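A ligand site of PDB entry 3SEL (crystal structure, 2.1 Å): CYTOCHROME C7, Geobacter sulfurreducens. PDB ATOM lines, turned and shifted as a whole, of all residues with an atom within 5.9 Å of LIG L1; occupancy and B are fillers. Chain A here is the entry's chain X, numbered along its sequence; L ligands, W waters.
FE1 of LIG L1 is bound by NE2 of His 17 (2.0 Å). A ring nitrogen (NE2) of His 31 binds an iron atom (FE1) of LIG L1, 2.0 Å away. FE1 of LG2 L2 is bound by NE2 of His 20 (2.0 Å). A carbon (C25) of LIG L1 is covalently linked to the side-chain sulfur of Cys 30. C18 of LIG L1 is bonded to SG of Cys 27 (2.0 Å).
OD1 of Asp 3 is in hydrogen-bond range of N of His 17 (3.0 Å). O of Pro 16 sits at hydrogen-bond distance from ND1 of His 20. ND1 of His 17 sits close to NE2 of Gln 21 (3.4 Å). O of Ile 4 is in hydrogen-bond range of N of Phe 15 (2.9 Å).
An oxygen (O3) of LIG L1 lies close to the backbone carbonyl oxygen of Asp 2 (3.3 Å). Residues that only touch LIG L1: Ile 4, Gln 21, Asp 3, Phe 15, Pro 25, Val 24, His 20 and Ala 1. 13 residues have an atom within 4 Å of LIG L1: Ala 1, Asp 2, Asp 3, Ile 4, Phe 15, His 17, His 20, Gln 21, Val 24, Pro 25, Cys 27, Cys 30 and His 31. The nearest printed residue that does not touch LIG L1 is Asp 26 (4.7 Å).
Water W2 lies within hydrogen-bond range of a ring nitrogen (ND1) of His 17 and an oxygen (O2) of LIG L1.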
ATOM      1  N   ALA A   1       1.165  -5.737  11.188  1.00  0.00           N
ATOM      2  CA  ALA A   1       2.316  -5.788  10.261  1.00  0.00           C
ATOM      3  C   ALA A   1       2.605  -7.247   9.998  1.00  0.00           C
ATOM      4  O   ALA A   1       2.055  -8.121  10.653  1.00  0.00           O
ATOM      5  CB  ALA A   1       3.510  -5.131  10.857  1.00  0.00           C
ATOM      6  N   ASP A   2       3.437  -7.498   9.018  1.00  0.00           N
ATOM      7  CA  ASP A   2       3.691  -8.845   8.573  1.00  0.00           C
ATOM      8  C   ASP A   2       4.918  -9.335   9.269  1.00  0.00           C
ATOM      9  O   ASP A   2       5.778  -8.536   9.637  1.00  0.00           O
ATOM     10  CB  ASP A   2       3.924  -8.858   7.068  1.00  0.00           C
ATOM     11  CG  ASP A   2       2.671  -8.573   6.318  1.00  0.00           C
ATOM     12  OD1 ASP A   2       1.675  -9.295   6.617  1.00  0.00           O
ATOM     13  OD2 ASP A   2       2.580  -7.659   5.439  1.00  0.00           O
ATOM     14  N   ASP A   3       4.979 -10.650   9.452  1.00  0.00           N
ATOM     15  CA  ASP A   3       6.213 -11.345   9.788  1.00  0.00           C
ATOM     16  C   ASP A   3       7.307 -11.114   8.756  1.00  0.00           C
ATOM     17  O   ASP A   3       7.019 -10.764   7.619  1.00  0.00           O
ATOM     18  CB  ASP A   3       5.972 -12.848   9.920  1.00  0.00           C
ATOM     19  CG  ASP A   3       5.164 -13.190  11.139  1.00  0.00           C
ATOM     20  OD1 ASP A   3       4.996 -12.356  12.062  1.00  0.00           O
ATOM     21  OD2 ASP A   3       4.650 -14.285  11.247  1.00  0.00           O
ATOM     22  N   ILE A   4       8.542 -11.268   9.199  1.00  0.00           N
ATOM     23  CA  ILE A   4       9.718 -11.068   8.362  1.00  0.00           C
ATOM     24  C   ILE A   4      10.457 -12.377   8.187  1.00  0.00           C
ATOM     25  O   ILE A   4      10.365 -13.262   9.025  1.00  0.00           O
ATOM     26  CB  ILE A   4      10.685 -10.078   9.069  1.00  0.00           C
ATOM     27  CG1 ILE A   4      10.123  -8.672   9.044  1.00  0.00           C
ATOM     28  CG2 ILE A   4      12.112 -10.077   8.431  1.00  0.00           C
ATOM     29  CD1 ILE A   4      10.940  -7.733   9.813  1.00  0.00           C
ATOM     30  N   PHE A  15      10.658 -15.243  11.191  1.00  0.00           N
ATOM     31  CA  PHE A  15      10.457 -14.645  12.493  1.00  0.00           C
ATOM     32  C   PHE A  15       8.943 -14.423  12.696  1.00  0.00           C
ATOM     33  O   PHE A  15       8.385 -13.476  12.185  1.00  0.00           O
ATOM     34  CB  PHE A  15      11.217 -13.332  12.615  1.00  0.00           C
ATOM     35  CG  PHE A  15      11.016 -12.683  13.945  1.00  0.00           C
ATOM     36  CD1 PHE A  15      11.623 -13.222  15.072  1.00  0.00           C
ATOM     37  CD2 PHE A  15      10.110 -11.653  14.086  1.00  0.00           C
ATOM     38  CE1 PHE A  15      11.397 -12.690  16.314  1.00  0.00           C
ATOM     39  CE2 PHE A  15       9.865 -11.105  15.348  1.00  0.00           C
ATOM     40  CZ  PHE A  15      10.511 -11.618  16.455  1.00  0.00           C
ATOM     41  N   PRO A  16       8.290 -15.336  13.409  1.00  0.00           N
ATOM     42  CA  PRO A  16       6.860 -15.188  13.746  1.00  0.00           C
ATOM     43  C   PRO A  16       6.647 -14.302  14.987  1.00  0.00           C
ATOM     44  O   PRO A  16       6.934 -14.698  16.153  1.00  0.00           O
ATOM     45  CB  PRO A  16       6.403 -16.642  13.949  1.00  0.00           C
ATOM     46  CG  PRO A  16       7.635 -17.324  14.466  1.00  0.00           C
ATOM     47  CD  PRO A  16       8.836 -16.611  13.903  1.00  0.00           C
ATOM     48  N   HIS A  17       6.159 -13.081  14.742  1.00  0.00           N
ATOM     49  CA  HIS A  17       6.026 -12.120  15.816  1.00  0.00           C
ATOM     50  C   HIS A  17       4.969 -12.488  16.893  1.00  0.00           C
ATOM     51  O   HIS A  17       5.210 -12.294  18.072  1.00  0.00           O
ATOM     52  CB  HIS A  17       5.685 -10.712  15.302  1.00  0.00           C
ATOM     53  CG  HIS A  17       5.682  -9.689  16.383  1.00  0.00           C
ATOM     54  ND1 HIS A  17       4.517  -9.146  16.888  1.00  0.00           N
ATOM     55  CD2 HIS A  17       6.694  -9.131  17.085  1.00  0.00           C
ATOM     56  CE1 HIS A  17       4.822  -8.291  17.842  1.00  0.00           C
ATOM     57  NE2 HIS A  17       6.140  -8.254  17.975  1.00  0.00           N
ATOM     58  N   HIS A  20       6.232 -14.654  19.624  1.00  0.00           N
ATOM     59  CA  HIS A  20       7.149 -13.935  20.469  1.00  0.00           C
ATOM     60  C   HIS A  20       6.442 -12.970  21.440  1.00  0.00           C
ATOM     61  O   HIS A  20       6.802 -12.895  22.596  1.00  0.00           O
ATOM     62  CB  HIS A  20       8.200 -13.228  19.623  1.00  0.00           C
ATOM     63  CG  HIS A  20       9.194 -14.164  19.018  1.00  0.00           C
ATOM     64  ND1 HIS A  20       8.978 -14.782  17.820  1.00  0.00           N
ATOM     65  CD2 HIS A  20      10.356 -14.669  19.500  1.00  0.00           C
ATOM     66  CE1 HIS A  20       9.975 -15.604  17.556  1.00  0.00           C
ATOM     67  NE2 HIS A  20      10.812 -15.579  18.570  1.00  0.00           N
ATOM     68  N   GLN A  21       5.454 -12.239  20.951  1.00  0.00           N
ATOM     69  CA  GLN A  21       4.632 -11.395  21.779  1.00  0.00           C
ATOM     70  C   GLN A  21       3.997 -12.186  22.948  1.00  0.00           C
ATOM     71  O   GLN A  21       4.056 -11.769  24.086  1.00  0.00           O
ATOM     72  CB  GLN A  21       3.544 -10.808  20.884  1.00  0.00           C
ATOM     73  CG  GLN A  21       2.916  -9.543  21.357  1.00  0.00           C
ATOM     74  CD  GLN A  21       2.397  -8.703  20.155  1.00  0.00           C
ATOM     75  OE1 GLN A  21       2.420  -7.481  20.183  1.00  0.00           O
ATOM     76  NE2 GLN A  21       1.929  -9.375  19.133  1.00  0.00           N
ATOM     77  N   LYS A  22       3.478 -13.366  22.619  1.00  0.00           N
ATOM     78  CA  LYS A  22       2.904 -14.291  23.581  1.00  0.00           C
ATOM     79  C   LYS A  22       3.909 -14.873  24.574  1.00  0.00           C
ATOM     80  O   LYS A  22       3.660 -14.890  25.789  1.00  0.00           O
ATOM     81  CB  LYS A  22       2.216 -15.433  22.802  1.00  0.00           C
ATOM     82  CG  LYS A  22       1.536 -16.440  23.707  1.00  0.00           C
ATOM     83  N   VAL A  24       7.209 -13.918  25.180  1.00  0.00           N
ATOM     84  CA  VAL A  24       8.138 -12.992  25.787  1.00  0.00           C
ATOM     85  C   VAL A  24       7.391 -11.675  26.031  1.00  0.00           C
ATOM     86  O   VAL A  24       7.587 -10.654  25.344  1.00  0.00           O
ATOM     87  CB  VAL A  24       9.423 -12.751  24.921  1.00  0.00           C
ATOM     88  CG1 VAL A  24      10.462 -11.978  25.711  1.00  0.00           C
ATOM     89  CG2 VAL A  24       9.993 -14.066  24.393  1.00  0.00           C
ATOM     90  N   PRO A  25       6.496 -11.721  27.018  1.00  0.00           N
ATOM     91  CA  PRO A  25       5.695 -10.548  27.368  1.00  0.00           C
ATOM     92  C   PRO A  25       6.519  -9.353  27.833  1.00  0.00           C
ATOM     93  O   PRO A  25       6.076  -8.213  27.732  1.00  0.00           O
ATOM     94  CB  PRO A  25       4.750 -11.080  28.463  1.00  0.00           C
ATOM     95  CG  PRO A  25       5.401 -12.349  28.938  1.00  0.00           C
ATOM     96  CD  PRO A  25       6.116 -12.923  27.785  1.00  0.00           C
ATOM     97  N   ASP A  26       7.720  -9.590  28.305  1.00  0.00           N
ATOM     98  CA  ASP A  26       8.652  -8.524  28.500  1.00  0.00           C
ATOM     99  C   ASP A  26       9.167  -7.923  27.158  1.00  0.00           C
ATOM    100  O   ASP A  26      10.249  -8.280  26.635  1.00  0.00           O
ATOM    101  CB  ASP A  26       9.819  -9.028  29.352  1.00  0.00           C
ATOM    102  CG  ASP A  26      10.705  -7.898  29.795  1.00  0.00           C
ATOM    103  OD1 ASP A  26      10.379  -6.740  29.439  1.00  0.00           O
ATOM    104  OD2 ASP A  26      11.756  -8.079  30.427  1.00  0.00           O
ATOM    105  N   CYS A  27       8.413  -6.964  26.642  1.00  0.00           N
ATOM    106  CA  CYS A  27       8.656  -6.402  25.311  1.00  0.00           C
ATOM    107  C   CYS A  27      10.013  -5.768  25.160  1.00  0.00           C
ATOM    108  O   CYS A  27      10.594  -5.767  24.051  1.00  0.00           O
ATOM    109  CB  CYS A  27       7.593  -5.372  24.989  1.00  0.00           C
ATOM    110  SG  CYS A  27       5.915  -5.978  25.256  1.00  0.00           S
ATOM    111  N   LYS A  28      10.523  -5.262  26.258  1.00  0.00           N
ATOM    112  CA  LYS A  28      11.820  -4.589  26.267  1.00  0.00           C
ATOM    113  C   LYS A  28      13.010  -5.509  25.964  1.00  0.00           C
ATOM    114  O   LYS A  28      14.120  -5.031  25.752  1.00  0.00           O
ATOM    115  CB  LYS A  28      12.012  -3.867  27.606  1.00  0.00           C
ATOM    116  CG  LYS A  28      11.112  -2.650  27.741  1.00  0.00           C
ATOM    117  CD  LYS A  28      11.575  -1.675  28.847  1.00  0.00           C
ATOM    118  CE  LYS A  28      12.778  -0.871  28.410  1.00  0.00           C
ATOM    119  NZ  LYS A  28      13.332  -0.147  29.564  1.00  0.00           N
ATOM    120  N   LYS A  29      12.780  -6.824  25.935  1.00  0.00           N
ATOM    121  CA  LYS A  29      13.822  -7.741  25.425  1.00  0.00           C
ATOM    122  C   LYS A  29      14.133  -7.400  23.974  1.00  0.00           C
ATOM    123  O   LYS A  29      15.228  -7.563  23.532  1.00  0.00           O
ATOM    124  CB  LYS A  29      13.379  -9.204  25.545  1.00  0.00           C
ATOM    125  CG  LYS A  29      13.362  -9.723  26.960  1.00  0.00           C
ATOM    126  CD  LYS A  29      14.785 -10.133  27.394  1.00  0.00           C
ATOM    127  CE  LYS A  29      14.925 -10.255  28.909  1.00  0.00           C
ATOM    128  N   CYS A  30      13.165  -6.889  23.236  1.00  0.00           N
ATOM    129  CA  CYS A  30      13.422  -6.525  21.843  1.00  0.00           C
ATOM    130  C   CYS A  30      13.192  -5.084  21.451  1.00  0.00           C
ATOM    131  O   CYS A  30      13.864  -4.578  20.549  1.00  0.00           O
ATOM    132  CB  CYS A  30      12.586  -7.421  20.931  1.00  0.00           C
ATOM    133  SG  CYS A  30      13.010  -9.190  21.074  1.00  0.00           S
ATOM    134  N   HIS A  31      12.229  -4.449  22.113  1.00  0.00           N
ATOM    135  CA  HIS A  31      11.797  -3.107  21.757  1.00  0.00           C
ATOM    136  C   HIS A  31      12.380  -2.024  22.669  1.00  0.00           C
ATOM    137  O   HIS A  31      12.777  -2.313  23.766  1.00  0.00           O
ATOM    138  CB  HIS A  31      10.270  -3.086  21.756  1.00  0.00           C
ATOM    139  CG  HIS A  31       9.675  -3.892  20.643  1.00  0.00           C
ATOM    140  ND1 HIS A  31      10.026  -3.697  19.323  1.00  0.00           N
ATOM    141  CD2 HIS A  31       8.763  -4.897  20.646  1.00  0.00           C
ATOM    142  CE1 HIS A  31       9.347  -4.547  18.571  1.00  0.00           C
ATOM    143  NE2 HIS A  31       8.565  -5.275  19.344  1.00  0.00           N
HETATM  144 FE1  LIG L   1       7.385  -6.799  18.700  1.00  0.00          FE
HETATM  145  C1  LIG L   1       6.772  -5.711  15.507  1.00  0.00           C
HETATM  146  C2  LIG L   1       4.932  -4.811  19.861  1.00  0.00           C
HETATM  147  C3  LIG L   1       7.539  -8.381  21.749  1.00  0.00           C
HETATM  148  C4  LIG L   1      10.339  -8.105  17.806  1.00  0.00           C
HETATM  149  N1  LIG L   1       6.168  -5.479  17.846  1.00  0.00           N
HETATM  150  C5  LIG L   1       5.963  -5.263  16.507  1.00  0.00           C
HETATM  151  C6  LIG L   1       4.749  -4.488  16.358  1.00  0.00           C
HETATM  152  C7  LIG L   1       4.247  -4.225  17.557  1.00  0.00           C
HETATM  153  C8  LIG L   1       5.131  -4.845  18.511  1.00  0.00           C
HETATM  154  C9  LIG L   1       2.955  -3.416  17.898  1.00  0.00           C
HETATM  155  C10 LIG L   1       4.120  -4.063  15.028  1.00  0.00           C
HETATM  156  C11 LIG L   1       3.161  -5.189  14.581  1.00  0.00           C
HETATM  157  C12 LIG L   1       2.476  -5.955  15.717  1.00  0.00           C
HETATM  158  O1  LIG L   1       3.080  -6.246  16.793  1.00  0.00           O
HETATM  159  O2  LIG L   1       1.280  -6.334  15.593  1.00  0.00           O
HETATM  160  N2  LIG L   1       6.384  -6.685  20.480  1.00  0.00           N
HETATM  161  C13 LIG L   1       5.406  -5.753  20.745  1.00  0.00           C
HETATM  162  C14 LIG L   1       5.004  -5.914  22.130  1.00  0.00           C
HETATM  163  C15 LIG L   1       5.730  -6.918  22.642  1.00  0.00           C
HETATM  164  C16 LIG L   1       6.592  -7.411  21.621  1.00  0.00           C
HETATM  165  C17 LIG L   1       3.904  -5.075  22.812  1.00  0.00           C
HETATM  166  C18 LIG L   1       5.675  -7.535  24.060  1.00  0.00           C
HETATM  167  C19 LIG L   1       4.469  -7.944  24.499  1.00  0.00           C
HETATM  168  N3  LIG L   1       8.679  -7.964  19.594  1.00  0.00           N
HETATM  169  C20 LIG L   1       8.563  -8.553  20.847  1.00  0.00           C
HETATM  170  C21 LIG L   1       9.705  -9.414  21.052  1.00  0.00           C
HETATM  171  C22 LIG L   1      10.479  -9.359  19.973  1.00  0.00           C
HETATM  172  C23 LIG L   1       9.850  -8.443  19.038  1.00  0.00           C
HETATM  173  C24 LIG L   1       9.903 -10.203  22.376  1.00  0.00           C
HETATM  174  C25 LIG L   1      11.818 -10.106  19.721  1.00  0.00           C
HETATM  175  C26 LIG L   1      11.929 -11.436  20.036  1.00  0.00           C
HETATM  176  N4  LIG L   1       8.406  -6.850  16.950  1.00  0.00           N
HETATM  177  C27 LIG L   1       9.621  -7.480  16.835  1.00  0.00           C
HETATM  178  C28 LIG L   1      10.020  -7.398  15.464  1.00  0.00           C
HETATM  179  C29 LIG L   1       8.929  -6.638  14.735  1.00  0.00           C
HETATM  180  C30 LIG L   1       7.945  -6.372  15.736  1.00  0.00           C
HETATM  181  C31 LIG L   1      11.313  -7.917  14.870  1.00  0.00           C
HETATM  182  C32 LIG L   1       8.862  -6.327  13.221  1.00  0.00           C
HETATM  183  C33 LIG L   1       8.753  -7.679  12.462  1.00  0.00           C
HETATM  184  C34 LIG L   1       7.441  -8.407  12.641  1.00  0.00           C
HETATM  185  O3  LIG L   1       6.381  -7.753  12.766  1.00  0.00           O
HETATM  186  O4  LIG L   1       7.426  -9.671  12.647  1.00  0.00           O
HETATM  187 FE1  LG2 L   2      12.294 -16.871  19.034  1.00  0.00          FE
HETATM  188  C1  LG2 L   2       9.888 -19.196  19.388  1.00  0.00           C
HETATM  189  C2  LG2 L   2      12.600 -17.702  15.687  1.00  0.00           C
HETATM  190  C3  LG2 L   2      14.530 -14.337  18.605  1.00  0.00           C
HETATM  191  C4  LG2 L   2      12.244 -16.190  22.412  1.00  0.00           C
HETATM  192  N1  LG2 L   2      11.425 -18.215  17.755  1.00  0.00           N
HETATM  193  C5  LG2 L   2      10.408 -19.026  18.108  1.00  0.00           C
HETATM  194  C6  LG2 L   2       9.996 -19.724  16.923  1.00  0.00           C
HETATM  195  C7  LG2 L   2      10.728 -19.322  15.901  1.00  0.00           C
HETATM  196  C8  LG2 L   2      11.651 -18.355  16.408  1.00  0.00           C
HETATM  197  C9  LG2 L   2      10.601 -19.798  14.436  1.00  0.00           C
HETATM  198  C10 LG2 L   2       8.900 -20.806  16.853  1.00  0.00           C
HETATM  199  C11 LG2 L   2       7.523 -20.194  16.986  1.00  0.00           C
HETATM  200  C12 LG2 L   2       6.501 -21.303  17.099  1.00  0.00           C
HETATM  201  O1  LG2 L   2       6.855 -22.439  17.520  1.00  0.00           O
HETATM  202  O2  LG2 L   2       5.318 -21.042  16.770  1.00  0.00           O
HETATM  203  N2  LG2 L   2      13.357 -16.194  17.473  1.00  0.00           N
HETATM  204  C13 LG2 L   2      13.359 -16.665  16.179  1.00  0.00           C
HETATM  205  C14 LG2 L   2      14.254 -15.885  15.387  1.00  0.00           C
HETATM  206  C15 LG2 L   2      14.769 -14.939  16.170  1.00  0.00           C
HETATM  207  C16 LG2 L   2      14.220 -15.104  17.498  1.00  0.00           C
HETATM  208  C17 LG2 L   2      14.516 -16.161  13.875  1.00  0.00           C
HETATM  209  C18 LG2 L   2      15.776 -13.857  15.743  1.00  0.00           C
HETATM  210  C19 LG2 L   2      15.450 -13.128  14.637  1.00  0.00           C
HETATM  211  N3  LG2 L   2      13.245 -15.523  20.313  1.00  0.00           N
HETATM  212  C20 LG2 L   2      14.102 -14.542  19.895  1.00  0.00           C
HETATM  213  C21 LG2 L   2      14.481 -13.739  21.050  1.00  0.00           C
HETATM  214  C22 LG2 L   2      13.827 -14.241  22.105  1.00  0.00           C
HETATM  215  C23 LG2 L   2      13.054 -15.393  21.650  1.00  0.00           C
HETATM  216  C24 LG2 L   2      15.448 -12.514  20.976  1.00  0.00           C
HETATM  217  C25 LG2 L   2      13.838 -13.736  23.563  1.00  0.00           C
HETATM  218  C26 LG2 L   2      14.102 -12.429  23.831  1.00  0.00           C
HETATM  219  N4  LG2 L   2      11.230 -17.546  20.637  1.00  0.00           N
HETATM  220  C27 LG2 L   2      11.433 -17.197  21.969  1.00  0.00           C
HETATM  221  C28 LG2 L   2      10.650 -18.065  22.814  1.00  0.00           C
HETATM  222  C29 LG2 L   2       9.928 -19.000  21.877  1.00  0.00           C
HETATM  223  C30 LG2 L   2      10.316 -18.590  20.543  1.00  0.00           C
HETATM  224  C31 LG2 L   2      10.565 -18.100  24.348  1.00  0.00           C
HETATM  225  C32 LG2 L   2       8.951 -20.133  22.244  1.00  0.00           C
HETATM  226  C33 LG2 L   2       7.597 -19.727  21.695  1.00  0.00           C
HETATM  227  C34 LG2 L   2       6.722 -20.910  21.330  1.00  0.00           C
HETATM  228  O3  LG2 L   2       7.228 -22.049  21.070  1.00  0.00           O
HETATM  229  O4  LG2 L   2       5.478 -20.675  21.291  1.00  0.00           O
HETATM  230  C1  LG3 L   3      17.547  -7.076  10.444  1.00  0.00           C
HETATM  231  C2  LG3 L   3      16.836  -8.199  11.183  1.00  0.00           C
HETATM  232  C3  LG3 L   3      15.434  -7.728  11.682  1.00  0.00           C
HETATM  233  C4  LG3 L   3      15.532  -6.512  12.632  1.00  0.00           C
HETATM  234  C5  LG3 L   3      16.362  -5.402  11.968  1.00  0.00           C
HETATM  235  C6  LG3 L   3      17.719  -5.903  11.419  1.00  0.00           C
HETATM  236  C7  LG3 L   3      14.676  -8.918  12.315  1.00  0.00           C
HETATM  237  C8  LG3 L   3      15.214  -9.348  13.680  1.00  0.00           C
HETATM  238  C9  LG3 L   3      15.330  -8.099  14.621  1.00  0.00           C
HETATM  239  C10 LG3 L   3      16.109  -6.939  13.970  1.00  0.00           C
HETATM  240  C11 LG3 L   3      16.084  -8.457  15.921  1.00  0.00           C
HETATM  241  C12 LG3 L   3      16.075  -7.292  16.943  1.00  0.00           C
HETATM  242  C13 LG3 L   3      16.843  -6.115  16.343  1.00  0.00           C
HETATM  243  C14 LG3 L   3      16.282  -5.738  14.968  1.00  0.00           C
HETATM  244  C15 LG3 L   3      15.499  -9.623  16.724  1.00  0.00           C
HETATM  245  C16 LG3 L   3      16.054  -9.396  18.136  1.00  0.00           C
HETATM  246  C17 LG3 L   3      16.755  -7.997  18.115  1.00  0.00           C
HETATM  247  C18 LG3 L   3      14.159  -5.883  12.832  1.00  0.00           C
HETATM  248  C19 LG3 L   3      16.623  -7.362  19.504  1.00  0.00           C
HETATM  249  O1  LG3 L   3      18.212  -6.443  16.185  1.00  0.00           O
HETATM  250  O2  LG3 L   3      18.823  -7.476   9.928  1.00  0.00           O
HETATM  251  C20 LG3 L   3      14.635  -6.914  17.252  1.00  0.00           C
HETATM  252  C21 LG3 L   3      16.988  -8.375  20.603  1.00  0.00           C
HETATM  253  C22 LG3 L   3      18.419  -8.855  20.499  1.00  0.00           C
HETATM  254  C23 LG3 L   3      19.396  -7.910  21.200  1.00  0.00           C
HETATM  255  O3  LG3 L   3      19.436  -7.854  22.436  1.00  0.00           O
HETATM  256  O4  LG3 L   3      20.135  -7.190  20.526  1.00  0.00           O
HETATM  257  C24 LG3 L   3      17.409  -6.048  19.727  1.00  0.00           C
HETATM  258  O   HOH W   1       4.364  -9.269  12.721  1.00  0.00           O
HETATM  259  O   HOH W   2       2.233  -9.495  15.331  1.00  0.00           O
